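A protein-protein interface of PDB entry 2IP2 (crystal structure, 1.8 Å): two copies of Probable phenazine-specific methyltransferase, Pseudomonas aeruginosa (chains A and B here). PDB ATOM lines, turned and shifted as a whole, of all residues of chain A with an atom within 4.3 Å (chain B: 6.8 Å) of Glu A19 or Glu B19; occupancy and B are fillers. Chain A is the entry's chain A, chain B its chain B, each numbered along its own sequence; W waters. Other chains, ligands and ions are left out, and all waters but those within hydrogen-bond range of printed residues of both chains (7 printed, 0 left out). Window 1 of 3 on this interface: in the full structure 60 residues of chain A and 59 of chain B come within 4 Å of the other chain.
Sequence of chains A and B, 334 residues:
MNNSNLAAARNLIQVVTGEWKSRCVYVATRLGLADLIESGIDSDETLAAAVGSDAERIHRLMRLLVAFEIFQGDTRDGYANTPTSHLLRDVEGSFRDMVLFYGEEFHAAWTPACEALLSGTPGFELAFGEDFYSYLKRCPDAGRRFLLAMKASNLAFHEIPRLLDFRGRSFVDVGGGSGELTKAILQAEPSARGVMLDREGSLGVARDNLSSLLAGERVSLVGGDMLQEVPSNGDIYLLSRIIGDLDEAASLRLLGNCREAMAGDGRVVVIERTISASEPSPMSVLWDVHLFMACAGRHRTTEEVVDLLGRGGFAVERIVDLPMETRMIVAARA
O of Val A16 lies within hydrogen-bond range of OG of Ser B22 (3.2 Å). The backbone NH (N) of Glu A19 lies within hydrogen-bond range of the side-chain hydroxyl (OG) of Ser B22 (3.1 Å). The side-chain carboxylate (OE1) of Glu A19 lies within hydrogen-bond range of a ring nitrogen (ND1) of His B107. O of Val B15 sits at hydrogen-bond distance from OG of Ser A22, 2.8 Å away. The backbone carbonyl oxygen (O) of Val B16 sits at hydrogen-bond distance from the side-chain hydroxyl (OG) of Ser A22 (3.2 Å). The backbone NH of Glu B19 is in hydrogen-bond range of the side-chain hydroxyl of Ser A22. NE of Arg A23 lies within hydrogen-bond range of O of Trp B110 (3.1 Å). NH2 of Arg A23 lies within hydrogen-bond range of O of Thr B111. ND1 of His A107 is in hydrogen-bond range of OE1 of Glu B19 (2.8 Å). The side-chain hydroxyl (OG1) of Thr B111 lies within hydrogen-bond range of a ring nitrogen (NE2) of His A107, 2.8 Å away. The guanidinium group of Arg B23 sits at hydrogen-bond distance from the backbone carbonyl oxygen of Trp A110, at 3.1 Å. NE1 of Trp A110 lies close to NE1 of Trp B20.
The side-chain hydroxyl of Ser A22 lies within hydrogen-bond range of the backbone carbonyl oxygen of Gly A18, at 3.5 Å. NH1 of Arg A23 sits at hydrogen-bond distance from ND1 of His A107 (3.5 Å). The backbone carbonyl oxygen of Gly B18 sits at hydrogen-bond distance from the side-chain hydroxyl of Ser B22, 3.4 Å away. The guanidinium group of Arg B23 sits at hydrogen-bond distance from the backbone carbonyl oxygen of Gly B103 (2.9 Å). The guanidinium group (NH1) of Arg B23 lies within hydrogen-bond range of a ring nitrogen (ND1) of His B107 (3.5 Å). The side-chain hydroxyl (OG1) of Thr B111 lies within hydrogen-bond range of the backbone carbonyl oxygen (O) of His B107 (3.1 Å).
Among the printed residues, pairs that only touch across the chains: Trp A20 with Trp B110 (3.4 Å), Trp A20 with Tyr B102 (3.4 Å), Glu A19 with Glu B19 (3.6 Å), Thr A17 with Leu B286 (3.6 Å), Arg A23 with Glu B19 (3.6 Å), Glu A19 with Arg B23 (3.7 Å), His A107 with His B107 (3.7 Å), Trp A110 with Cys B24 (3.7 Å), Ser A22 with Gly B18 (3.8 Å), Lys A21 with Leu B286 (3.8 Å), Val A16 with Tyr B102 (3.9 Å), Gly A18 with Ser B22 (3.9 Å) and Trp A20 with Leu B286 (3.9 Å).
Of the printed residues of chain B, Val A16 touches Ser B22 (3.2 Å) and Tyr B102 (3.9 Å). Printed residues of chain B within 4 Å of Lys A21: Leu B286. Thr B17 touches none of the printed residues of chain A. Printed residues of chain A within 4 Å of Glu B19: Glu A19, Ser A22, Arg A23 and His A107. Of the printed residues of chain A, His B107 touches Glu A19 (2.9 Å) and His A107 (3.7 Å). Ala B108 touches none of the printed residues of chain A. The nearest printed residue of chain B that does not touch Glu A19 is Gly B18 (4.3 Å). The nearest printed residue of chain A that does not touch Thr B111 is Glu A19 (6.2 Å).
Of the 19 printed residues of chain B, 13 touch a printed residue of chain A. Hydrophobic or aromatic side chains of chain B within 4 Å of the printed part of chain A: Trp B20, Tyr B102, His B107, Trp B110 and Leu B286. Of the 10 printed residues of chain A, 10 touch a printed residue of chain B. Hydrophobic or aromatic side chains of chain A that line the printed part of chain B: Val A16, Trp A20, His A107 and Trp A110. Among the printed residues, 25 pairs touch across the chains.
Val A16 touches Ser B22, and with the chains exchanged Ser A22 touches Val B16. Gly A18 touches Ser B22, and with the chains exchanged Ser A22 touches Gly B18. Glu A19 touches its own counterpart, Glu B19. His A107 touches its own counterpart, His B107. Of the 25 pairs that touch across the chains among the printed residues, 16 have their exchanged pair printed and touching as well.
Water W5 bridges OE1 of Gln B14 (2.8 Å) and NZ of Lys A21 (2.8 Å). Water W6 lies within hydrogen-bond range of the backbone carbonyl oxygen of Val B15 (2.8 Å) and the backbone carbonyl oxygen of Gly A18 (2.9 Å). Water W2 bridges the side-chain carboxylate of Glu B19 (2.8 Å) and the guanidinium group of Arg A23 (3.1 Å). Water W7 lies within hydrogen-bond range of OE2 of Glu A19 (2.8 Å), O of Tyr B102 (2.8 Å) and NE1 of Trp A20 (3.0 Å). Water W4 lies within hydrogen-bond range of the side-chain carboxylate (OE1) of Glu A19 (2.8 Å) and the guanidinium group (NH1) of Arg B23 (2.8 Å). Water W1 lies within hydrogen-bond range of O of His B107, OE2 of Glu A19 and N of Thr B111.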
ATOM      1  N   VAL A  16      18.811  -3.825 -12.567  1.00  0.00           N
ATOM      2  CA  VAL A  16      18.627  -2.754 -11.585  1.00  0.00           C
ATOM      3  C   VAL A  16      18.455  -3.351 -10.173  1.00  0.00           C
ATOM      4  O   VAL A  16      19.041  -2.856  -9.222  1.00  0.00           O
ATOM      5  CB  VAL A  16      17.418  -1.898 -11.952  1.00  0.00           C
ATOM      6  CG1 VAL A  16      17.017  -0.899 -10.806  1.00  0.00           C
ATOM      7  CG2 VAL A  16      17.721  -1.097 -13.177  1.00  0.00           C
ATOM      8  N   THR A  17      17.730  -4.458 -10.071  1.00  0.00           N
ATOM      9  CA  THR A  17      17.386  -5.015  -8.735  1.00  0.00           C
ATOM     10  C   THR A  17      18.399  -6.057  -8.266  1.00  0.00           C
ATOM     11  O   THR A  17      18.337  -6.586  -7.091  1.00  0.00           O
ATOM     12  CB  THR A  17      15.988  -5.646  -8.691  1.00  0.00           C
ATOM     13  OG1 THR A  17      15.933  -6.731  -9.637  1.00  0.00           O
ATOM     14  CG2 THR A  17      14.833  -4.618  -9.024  1.00  0.00           C
ATOM     15  N   GLY A  18      19.358  -6.367  -9.141  1.00  0.00           N
ATOM     16  CA  GLY A  18      20.393  -7.318  -8.817  1.00  0.00           C
ATOM     17  C   GLY A  18      21.089  -6.914  -7.516  1.00  0.00           C
ATOM     18  O   GLY A  18      21.467  -7.791  -6.727  1.00  0.00           O
ATOM     19  N   GLU A  19      21.252  -5.615  -7.306  1.00  0.00           N
ATOM     20  CA  GLU A  19      21.941  -5.141  -6.075  1.00  0.00           C
ATOM     21  C   GLU A  19      21.216  -5.735  -4.815  1.00  0.00           C
ATOM     22  O   GLU A  19      21.830  -6.095  -3.830  1.00  0.00           O
ATOM     23  CB  GLU A  19      21.840  -3.631  -6.011  1.00  0.00           C
ATOM     24  CG  GLU A  19      22.321  -3.088  -4.612  1.00  0.00           C
ATOM     25  CD  GLU A  19      22.135  -1.588  -4.620  1.00  0.00           C
ATOM     26  OE1 GLU A  19      22.866  -0.993  -5.386  1.00  0.00           O
ATOM     27  OE2 GLU A  19      21.198  -1.073  -3.972  1.00  0.00           O
ATOM     28  N   TRP A  20      19.896  -5.843  -4.845  1.00  0.00           N
ATOM     29  CA  TRP A  20      19.215  -6.324  -3.612  1.00  0.00           C
ATOM     30  C   TRP A  20      19.561  -7.802  -3.310  1.00  0.00           C
ATOM     31  O   TRP A  20      19.641  -8.235  -2.119  1.00  0.00           O
ATOM     32  CB  TRP A  20      17.680  -6.141  -3.766  1.00  0.00           C
ATOM     33  CG  TRP A  20      17.256  -4.726  -4.212  1.00  0.00           C
ATOM     34  CD1 TRP A  20      17.978  -3.555  -4.107  1.00  0.00           C
ATOM     35  CD2 TRP A  20      15.987  -4.362  -4.735  1.00  0.00           C
ATOM     36  NE1 TRP A  20      17.226  -2.506  -4.564  1.00  0.00           N
ATOM     37  CE2 TRP A  20      16.006  -2.962  -4.967  1.00  0.00           C
ATOM     38  CE3 TRP A  20      14.837  -5.101  -5.090  1.00  0.00           C
ATOM     39  CZ2 TRP A  20      14.876  -2.239  -5.503  1.00  0.00           C
ATOM     40  CZ3 TRP A  20      13.701  -4.391  -5.606  1.00  0.00           C
ATOM     41  CH2 TRP A  20      13.762  -2.971  -5.853  1.00  0.00           C
ATOM     42  N   LYS A  21      19.721  -8.617  -4.374  1.00  0.00           N
ATOM     43  CA  LYS A  21      20.157  -9.984  -4.177  1.00  0.00           C
ATOM     44  C   LYS A  21      21.543  -9.990  -3.517  1.00  0.00           C
ATOM     45  O   LYS A  21      21.792 -10.828  -2.653  1.00  0.00           O
ATOM     46  CB  LYS A  21      20.221 -10.774  -5.501  1.00  0.00           C
ATOM     47  CG  LYS A  21      18.838 -10.950  -6.133  1.00  0.00           C
ATOM     48  CD  LYS A  21      18.844 -11.305  -7.696  1.00  0.00           C
ATOM     49  CE  LYS A  21      19.625 -12.613  -7.872  1.00  0.00           C
ATOM     50  NZ  LYS A  21      19.805 -12.879  -9.332  1.00  0.00           N
ATOM     51  N   SER A  22      22.465  -9.149  -3.995  1.00  0.00           N
ATOM     52  CA  SER A  22      23.810  -9.085  -3.343  1.00  0.00           C
ATOM     53  C   SER A  22      23.634  -8.793  -1.863  1.00  0.00           C
ATOM     54  O   SER A  22      24.274  -9.428  -1.008  1.00  0.00           O
ATOM     55  CB  SER A  22      24.714  -8.026  -3.976  1.00  0.00           C
ATOM     56  OG  SER A  22      24.665  -8.057  -5.399  1.00  0.00           O
ATOM     57  N   ARG A  23      22.719  -7.865  -1.546  1.00  0.00           N
ATOM     58  CA  ARG A  23      22.511  -7.475  -0.122  1.00  0.00           C
ATOM     59  C   ARG A  23      21.932  -8.659   0.637  1.00  0.00           C
ATOM     60  O   ARG A  23      22.354  -8.900   1.751  1.00  0.00           O
ATOM     61  CB  ARG A  23      21.630  -6.222   0.034  1.00  0.00           C
ATOM     62  CG  ARG A  23      22.156  -4.935  -0.661  1.00  0.00           C
ATOM     63  CD  ARG A  23      23.640  -4.694  -0.258  1.00  0.00           C
ATOM     64  NE  ARG A  23      23.737  -4.145   1.129  1.00  0.00           N
ATOM     65  CZ  ARG A  23      24.859  -4.091   1.826  1.00  0.00           C
ATOM     66  NH1 ARG A  23      25.970  -4.555   1.307  1.00  0.00           N
ATOM     67  NH2 ARG A  23      24.890  -3.546   3.027  1.00  0.00           N
ATOM     68  N   HIS A 107      31.046  -2.206  -0.962  1.00  0.00           N
ATOM     69  CA  HIS A 107      29.689  -1.598  -1.082  1.00  0.00           C
ATOM     70  C   HIS A 107      29.798  -0.077  -0.853  1.00  0.00           C
ATOM     71  O   HIS A 107      29.196   0.734  -1.578  1.00  0.00           O
ATOM     72  CB  HIS A 107      28.755  -2.192  -0.027  1.00  0.00           C
ATOM     73  CG  HIS A 107      27.382  -1.578  -0.019  1.00  0.00           C
ATOM     74  ND1 HIS A 107      26.406  -1.924  -0.933  1.00  0.00           N
ATOM     75  CD2 HIS A 107      26.821  -0.647   0.794  1.00  0.00           C
ATOM     76  CE1 HIS A 107      25.299  -1.221  -0.696  1.00  0.00           C
ATOM     77  NE2 HIS A 107      25.528  -0.440   0.350  1.00  0.00           N
ATOM     78  N   TRP A 110      31.488   1.468  -3.975  1.00  0.00           N
ATOM     79  CA  TRP A 110      30.659   1.519  -5.155  1.00  0.00           C
ATOM     80  C   TRP A 110      29.486   2.468  -5.038  1.00  0.00           C
ATOM     81  O   TRP A 110      28.705   2.655  -5.991  1.00  0.00           O
ATOM     82  CB  TRP A 110      30.191   0.098  -5.535  1.00  0.00           C
ATOM     83  CG  TRP A 110      31.100  -0.626  -6.397  1.00  0.00           C
ATOM     84  CD1 TRP A 110      32.061  -1.543  -6.040  1.00  0.00           C
ATOM     85  CD2 TRP A 110      31.099  -0.580  -7.839  1.00  0.00           C
ATOM     86  NE1 TRP A 110      32.679  -2.052  -7.183  1.00  0.00           N
ATOM     87  CE2 TRP A 110      32.089  -1.488  -8.288  1.00  0.00           C
ATOM     88  CE3 TRP A 110      30.363   0.165  -8.785  1.00  0.00           C
ATOM     89  CZ2 TRP A 110      32.380  -1.679  -9.635  1.00  0.00           C
ATOM     90  CZ3 TRP A 110      30.681  -0.010 -10.166  1.00  0.00           C
ATOM     91  CH2 TRP A 110      31.676  -0.927 -10.553  1.00  0.00           C
ATOM     92  N   GLN B  14      28.468 -14.200  -9.527  1.00  0.00           N
ATOM     93  CA  GLN B  14      27.502 -13.406 -10.303  1.00  0.00           C
ATOM     94  C   GLN B  14      26.573 -12.660  -9.338  1.00  0.00           C
ATOM     95  O   GLN B  14      26.276 -11.491  -9.524  1.00  0.00           O
ATOM     96  CB  GLN B  14      26.652 -14.326 -11.184  1.00  0.00           C
ATOM     97  CG  GLN B  14      25.815 -13.591 -12.274  1.00  0.00           C
ATOM     98  CD  GLN B  14      24.563 -12.857 -11.715  1.00  0.00           C
ATOM     99  OE1 GLN B  14      23.842 -13.377 -10.874  1.00  0.00           O
ATOM    100  NE2 GLN B  14      24.312 -11.674 -12.219  1.00  0.00           N
ATOM    101  N   VAL B  15      26.081 -13.385  -8.339  1.00  0.00           N
ATOM    102  CA  VAL B  15      25.064 -12.805  -7.437  1.00  0.00           C
ATOM    103  C   VAL B  15      25.737 -11.743  -6.561  1.00  0.00           C
ATOM    104  O   VAL B  15      25.191 -10.672  -6.379  1.00  0.00           O
ATOM    105  CB  VAL B  15      24.387 -13.904  -6.544  1.00  0.00           C
ATOM    106  CG1 VAL B  15      23.454 -13.239  -5.509  1.00  0.00           C
ATOM    107  CG2 VAL B  15      23.568 -14.784  -7.407  1.00  0.00           C
ATOM    108  N   VAL B  16      26.894 -12.090  -5.971  1.00  0.00           N
ATOM    109  CA  VAL B  16      27.678 -11.161  -5.115  1.00  0.00           C
ATOM    110  C   VAL B  16      28.018  -9.838  -5.836  1.00  0.00           C
ATOM    111  O   VAL B  16      27.838  -8.740  -5.269  1.00  0.00           O
ATOM    112  CB  VAL B  16      28.956 -11.867  -4.576  1.00  0.00           C
ATOM    113  CG1 VAL B  16      29.928 -10.831  -3.846  1.00  0.00           C
ATOM    114  CG2 VAL B  16      28.546 -13.089  -3.610  1.00  0.00           C
ATOM    115  N   THR B  17      28.423  -9.934  -7.112  1.00  0.00           N
ATOM    116  CA  THR B  17      28.847  -8.765  -7.824  1.00  0.00           C
ATOM    117  C   THR B  17      27.752  -8.111  -8.636  1.00  0.00           C
ATOM    118  O   THR B  17      28.014  -7.092  -9.254  1.00  0.00           O
ATOM    119  CB  THR B  17      30.032  -9.081  -8.758  1.00  0.00           C
ATOM    120  OG1 THR B  17      29.612 -10.048  -9.719  1.00  0.00           O
ATOM    121  CG2 THR B  17      31.281  -9.568  -7.972  1.00  0.00           C
ATOM    122  N   GLY B  18      26.543  -8.669  -8.604  1.00  0.00           N
ATOM    123  CA  GLY B  18      25.367  -8.082  -9.299  1.00  0.00           C
ATOM    124  C   GLY B  18      25.193  -6.633  -8.931  1.00  0.00           C
ATOM    125  O   GLY B  18      24.779  -5.819  -9.760  1.00  0.00           O
ATOM    126  N   GLU B  19      25.452  -6.287  -7.661  1.00  0.00           N
ATOM    127  CA  GLU B  19      25.296  -4.875  -7.282  1.00  0.00           C
ATOM    128  C   GLU B  19      26.141  -3.905  -8.128  1.00  0.00           C
ATOM    129  O   GLU B  19      25.727  -2.761  -8.407  1.00  0.00           O
ATOM    130  CB  GLU B  19      25.684  -4.746  -5.796  1.00  0.00           C
ATOM    131  CG  GLU B  19      26.057  -3.332  -5.339  1.00  0.00           C
ATOM    132  CD  GLU B  19      26.617  -3.324  -3.863  1.00  0.00           C
ATOM    133  OE1 GLU B  19      25.862  -3.798  -2.976  1.00  0.00           O
ATOM    134  OE2 GLU B  19      27.751  -2.793  -3.677  1.00  0.00           O
ATOM    135  N   TRP B  20      27.371  -4.326  -8.472  1.00  0.00           N
ATOM    136  CA  TRP B  20      28.243  -3.431  -9.262  1.00  0.00           C
ATOM    137  C   TRP B  20      27.663  -3.160 -10.638  1.00  0.00           C
ATOM    138  O   TRP B  20      27.673  -2.016 -11.078  1.00  0.00           O
ATOM    139  CB  TRP B  20      29.644  -4.001  -9.418  1.00  0.00           C
ATOM    140  CG  TRP B  20      30.299  -4.437  -8.087  1.00  0.00           C
ATOM    141  CD1 TRP B  20      29.976  -4.047  -6.798  1.00  0.00           C
ATOM    142  CD2 TRP B  20      31.389  -5.314  -7.988  1.00  0.00           C
ATOM    143  NE1 TRP B  20      30.825  -4.678  -5.905  1.00  0.00           N
ATOM    144  CE2 TRP B  20      31.703  -5.459  -6.613  1.00  0.00           C
ATOM    145  CE3 TRP B  20      32.165  -5.997  -8.949  1.00  0.00           C
ATOM    146  CZ2 TRP B  20      32.770  -6.259  -6.168  1.00  0.00           C
ATOM    147  CZ3 TRP B  20      33.231  -6.791  -8.511  1.00  0.00           C
ATOM    148  CH2 TRP B  20      33.509  -6.923  -7.123  1.00  0.00           C
ATOM    149  N   LYS B  21      27.060  -4.162 -11.267  1.00  0.00           N
ATOM    150  CA  LYS B  21      26.264  -3.920 -12.492  1.00  0.00           C
ATOM    151  C   LYS B  21      25.128  -2.953 -12.288  1.00  0.00           C
ATOM    152  O   LYS B  21      24.927  -2.067 -13.125  1.00  0.00           O
ATOM    153  CB  LYS B  21      25.700  -5.212 -13.085  1.00  0.00           C
ATOM    154  CG  LYS B  21      26.777  -6.223 -13.472  1.00  0.00           C
ATOM    155  CD  LYS B  21      26.162  -7.638 -13.780  1.00  0.00           C
ATOM    156  CE  LYS B  21      24.962  -7.604 -14.743  1.00  0.00           C
ATOM    157  NZ  LYS B  21      24.418  -9.011 -15.024  1.00  0.00           N
ATOM    158  N   SER B  22      24.398  -3.068 -11.153  1.00  0.00           N
ATOM    159  CA  SER B  22      23.352  -2.025 -10.843  1.00  0.00           C
ATOM    160  C   SER B  22      23.939  -0.633 -10.791  1.00  0.00           C
ATOM    161  O   SER B  22      23.402   0.287 -11.423  1.00  0.00           O
ATOM    162  CB  SER B  22      22.571  -2.318  -9.545  1.00  0.00           C
ATOM    163  OG  SER B  22      22.135  -3.708  -9.565  1.00  0.00           O
ATOM    164  N   ARG B  23      25.105  -0.501 -10.155  1.00  0.00           N
ATOM    165  CA  ARG B  23      25.717   0.796 -10.053  1.00  0.00           C
ATOM    166  C   ARG B  23      26.082   1.351 -11.418  1.00  0.00           C
ATOM    167  O   ARG B  23      25.860   2.551 -11.673  1.00  0.00           O
ATOM    168  CB  ARG B  23      26.935   0.802  -9.138  1.00  0.00           C
ATOM    169  CG  ARG B  23      26.694   0.289  -7.710  1.00  0.00           C
ATOM    170  CD  ARG B  23      25.439   1.017  -7.129  1.00  0.00           C
ATOM    171  NE  ARG B  23      25.709   2.408  -6.679  1.00  0.00           N
ATOM    172  CZ  ARG B  23      24.792   3.349  -6.472  1.00  0.00           C
ATOM    173  NH1 ARG B  23      23.470   3.130  -6.702  1.00  0.00           N
ATOM    174  NH2 ARG B  23      25.194   4.558  -6.048  1.00  0.00           N
ATOM    175  N   CYS B  24      26.640   0.492 -12.266  1.00  0.00           N
ATOM    176  CA  CYS B  24      27.085   0.907 -13.581  1.00  0.00           C
ATOM    177  C   CYS B  24      25.874   1.374 -14.461  1.00  0.00           C
ATOM    178  O   CYS B  24      25.992   2.344 -15.246  1.00  0.00           O
ATOM    179  CB  CYS B  24      27.758  -0.272 -14.237  1.00  0.00           C
ATOM    180  SG  CYS B  24      29.466  -0.534 -13.655  1.00  0.00           S
ATOM    181  N   TYR B 102      15.666   4.168  -7.677  1.00  0.00           N
ATOM    182  CA  TYR B 102      16.131   2.930  -7.093  1.00  0.00           C
ATOM    183  C   TYR B 102      17.613   2.999  -6.725  1.00  0.00           C
ATOM    184  O   TYR B 102      18.016   2.410  -5.715  1.00  0.00           O
ATOM    185  CB  TYR B 102      15.918   1.783  -8.080  1.00  0.00           C
ATOM    186  CG  TYR B 102      14.492   1.269  -8.058  1.00  0.00           C
ATOM    187  CD1 TYR B 102      13.419   2.119  -7.886  1.00  0.00           C
ATOM    188  CD2 TYR B 102      14.230  -0.092  -8.261  1.00  0.00           C
ATOM    189  CE1 TYR B 102      12.091   1.612  -7.878  1.00  0.00           C
ATOM    190  CE2 TYR B 102      12.948  -0.603  -8.210  1.00  0.00           C
ATOM    191  CZ  TYR B 102      11.887   0.267  -8.038  1.00  0.00           C
ATOM    192  OH  TYR B 102      10.594  -0.200  -8.059  1.00  0.00           O
ATOM    193  N   GLY B 103      18.409   3.661  -7.575  1.00  0.00           N
ATOM    194  CA  GLY B 103      19.891   3.808  -7.355  1.00  0.00           C
ATOM    195  C   GLY B 103      20.266   4.881  -6.326  1.00  0.00           C
ATOM    196  O   GLY B 103      21.451   5.054  -5.980  1.00  0.00           O
ATOM    197  N   PHE B 106      16.528   3.758  -2.826  1.00  0.00           N
ATOM    198  CA  PHE B 106      16.520   2.372  -2.448  1.00  0.00           C
ATOM    199  C   PHE B 106      17.919   1.714  -2.296  1.00  0.00           C
ATOM    200  O   PHE B 106      18.076   0.709  -1.603  1.00  0.00           O
ATOM    201  CB  PHE B 106      15.633   1.546  -3.368  1.00  0.00           C
ATOM    202  CG  PHE B 106      14.147   1.886  -3.253  1.00  0.00           C
ATOM    203  CD1 PHE B 106      13.588   2.324  -2.050  1.00  0.00           C
ATOM    204  CD2 PHE B 106      13.316   1.747  -4.377  1.00  0.00           C
ATOM    205  CE1 PHE B 106      12.238   2.609  -1.931  1.00  0.00           C
ATOM    206  CE2 PHE B 106      11.924   2.044  -4.263  1.00  0.00           C
ATOM    207  CZ  PHE B 106      11.396   2.469  -3.050  1.00  0.00           C
ATOM    208  N   HIS B 107      18.923   2.333  -2.895  1.00  0.00           N
ATOM    209  CA  HIS B 107      20.307   1.969  -2.654  1.00  0.00           C
ATOM    210  C   HIS B 107      20.618   2.260  -1.188  1.00  0.00           C
ATOM    211  O   HIS B 107      21.092   1.384  -0.422  1.00  0.00           O
ATOM    212  CB  HIS B 107      21.261   2.763  -3.582  1.00  0.00           C
ATOM    213  CG  HIS B 107      22.705   2.503  -3.284  1.00  0.00           C
ATOM    214  ND1 HIS B 107      23.325   1.347  -3.702  1.00  0.00           N
ATOM    215  CD2 HIS B 107      23.640   3.200  -2.579  1.00  0.00           C
ATOM    216  CE1 HIS B 107      24.591   1.350  -3.274  1.00  0.00           C
ATOM    217  NE2 HIS B 107      24.809   2.483  -2.629  1.00  0.00           N
ATOM    218  N   ALA B 108      20.249   3.471  -0.740  1.00  0.00           N
ATOM    219  CA  ALA B 108      20.442   3.844   0.676  1.00  0.00           C
ATOM    220  C   ALA B 108      19.633   2.922   1.629  1.00  0.00           C
ATOM    221  O   ALA B 108      20.146   2.473   2.702  1.00  0.00           O
ATOM    222  CB  ALA B 108      20.000   5.301   0.829  1.00  0.00           C
ATOM    223  N   TRP B 110      18.689  -0.204   1.130  1.00  0.00           N
ATOM    224  CA  TRP B 110      19.192  -1.561   1.197  1.00  0.00           C
ATOM    225  C   TRP B 110      20.592  -1.683   1.864  1.00  0.00           C
ATOM    226  O   TRP B 110      21.081  -2.789   2.070  1.00  0.00           O
ATOM    227  CB  TRP B 110      19.252  -2.160  -0.183  1.00  0.00           C
ATOM    228  CG  TRP B 110      17.941  -2.804  -0.543  1.00  0.00           C
ATOM    229  CD1 TRP B 110      16.891  -2.247  -1.174  1.00  0.00           C
ATOM    230  CD2 TRP B 110      17.588  -4.171  -0.254  1.00  0.00           C
ATOM    231  NE1 TRP B 110      15.879  -3.194  -1.310  1.00  0.00           N
ATOM    232  CE2 TRP B 110      16.288  -4.382  -0.761  1.00  0.00           C
ATOM    233  CE3 TRP B 110      18.264  -5.221   0.374  1.00  0.00           C
ATOM    234  CZ2 TRP B 110      15.629  -5.629  -0.703  1.00  0.00           C
ATOM    235  CZ3 TRP B 110      17.625  -6.505   0.448  1.00  0.00           C
ATOM    236  CH2 TRP B 110      16.310  -6.691  -0.113  1.00  0.00           C
ATOM    237  N   THR B 111      21.194  -0.562   2.184  1.00  0.00           N
ATOM    238  CA  THR B 111      22.520  -0.562   2.885  1.00  0.00           C
ATOM    239  C   THR B 111      22.372  -1.216   4.285  1.00  0.00           C
ATOM    240  O   THR B 111      23.060  -2.203   4.571  1.00  0.00           O
ATOM    241  CB  THR B 111      23.173   0.812   2.871  1.00  0.00           C
ATOM    242  OG1 THR B 111      23.508   1.155   1.522  1.00  0.00           O
ATOM    243  CG2 THR B 111      24.460   0.805   3.698  1.00  0.00           C
ATOM    244  N   LEU B 286      11.823 -11.652  -4.640  1.00  0.00           N
ATOM    245  CA  LEU B 286      12.737 -10.484  -4.480  1.00  0.00           C
ATOM    246  C   LEU B 286      11.906  -9.204  -4.198  1.00  0.00           C
ATOM    247  O   LEU B 286      12.250  -8.430  -3.271  1.00  0.00           O
ATOM    248  CB  LEU B 286      13.601 -10.319  -5.772  1.00  0.00           C
ATOM    249  CG  LEU B 286      14.680  -9.211  -5.706  1.00  0.00           C
ATOM    250  CD1 LEU B 286      15.529  -9.313  -4.455  1.00  0.00           C
ATOM    251  CD2 LEU B 286      15.621  -9.096  -6.952  1.00  0.00           C
HETATM  252  O   HOH W   1      22.150  -1.168  -1.118  1.00  0.00           O
HETATM  253  O   HOH W   2      26.572  -5.962  -1.368  1.00  0.00           O
HETATM  254  O   HOH W   3      27.445   0.186  -3.771  1.00  0.00           O
HETATM  255  O   HOH W   4      22.136   0.750  -7.497  1.00  0.00           O
HETATM  256  O   HOH W   5      22.123 -11.389 -10.041  1.00  0.00           O
HETATM  257  O   HOH W   6      23.030  -9.928  -7.931  1.00  0.00           O
HETATM  258  O   HOH W   7      18.940  -0.242  -5.424  1.00  0.00           O
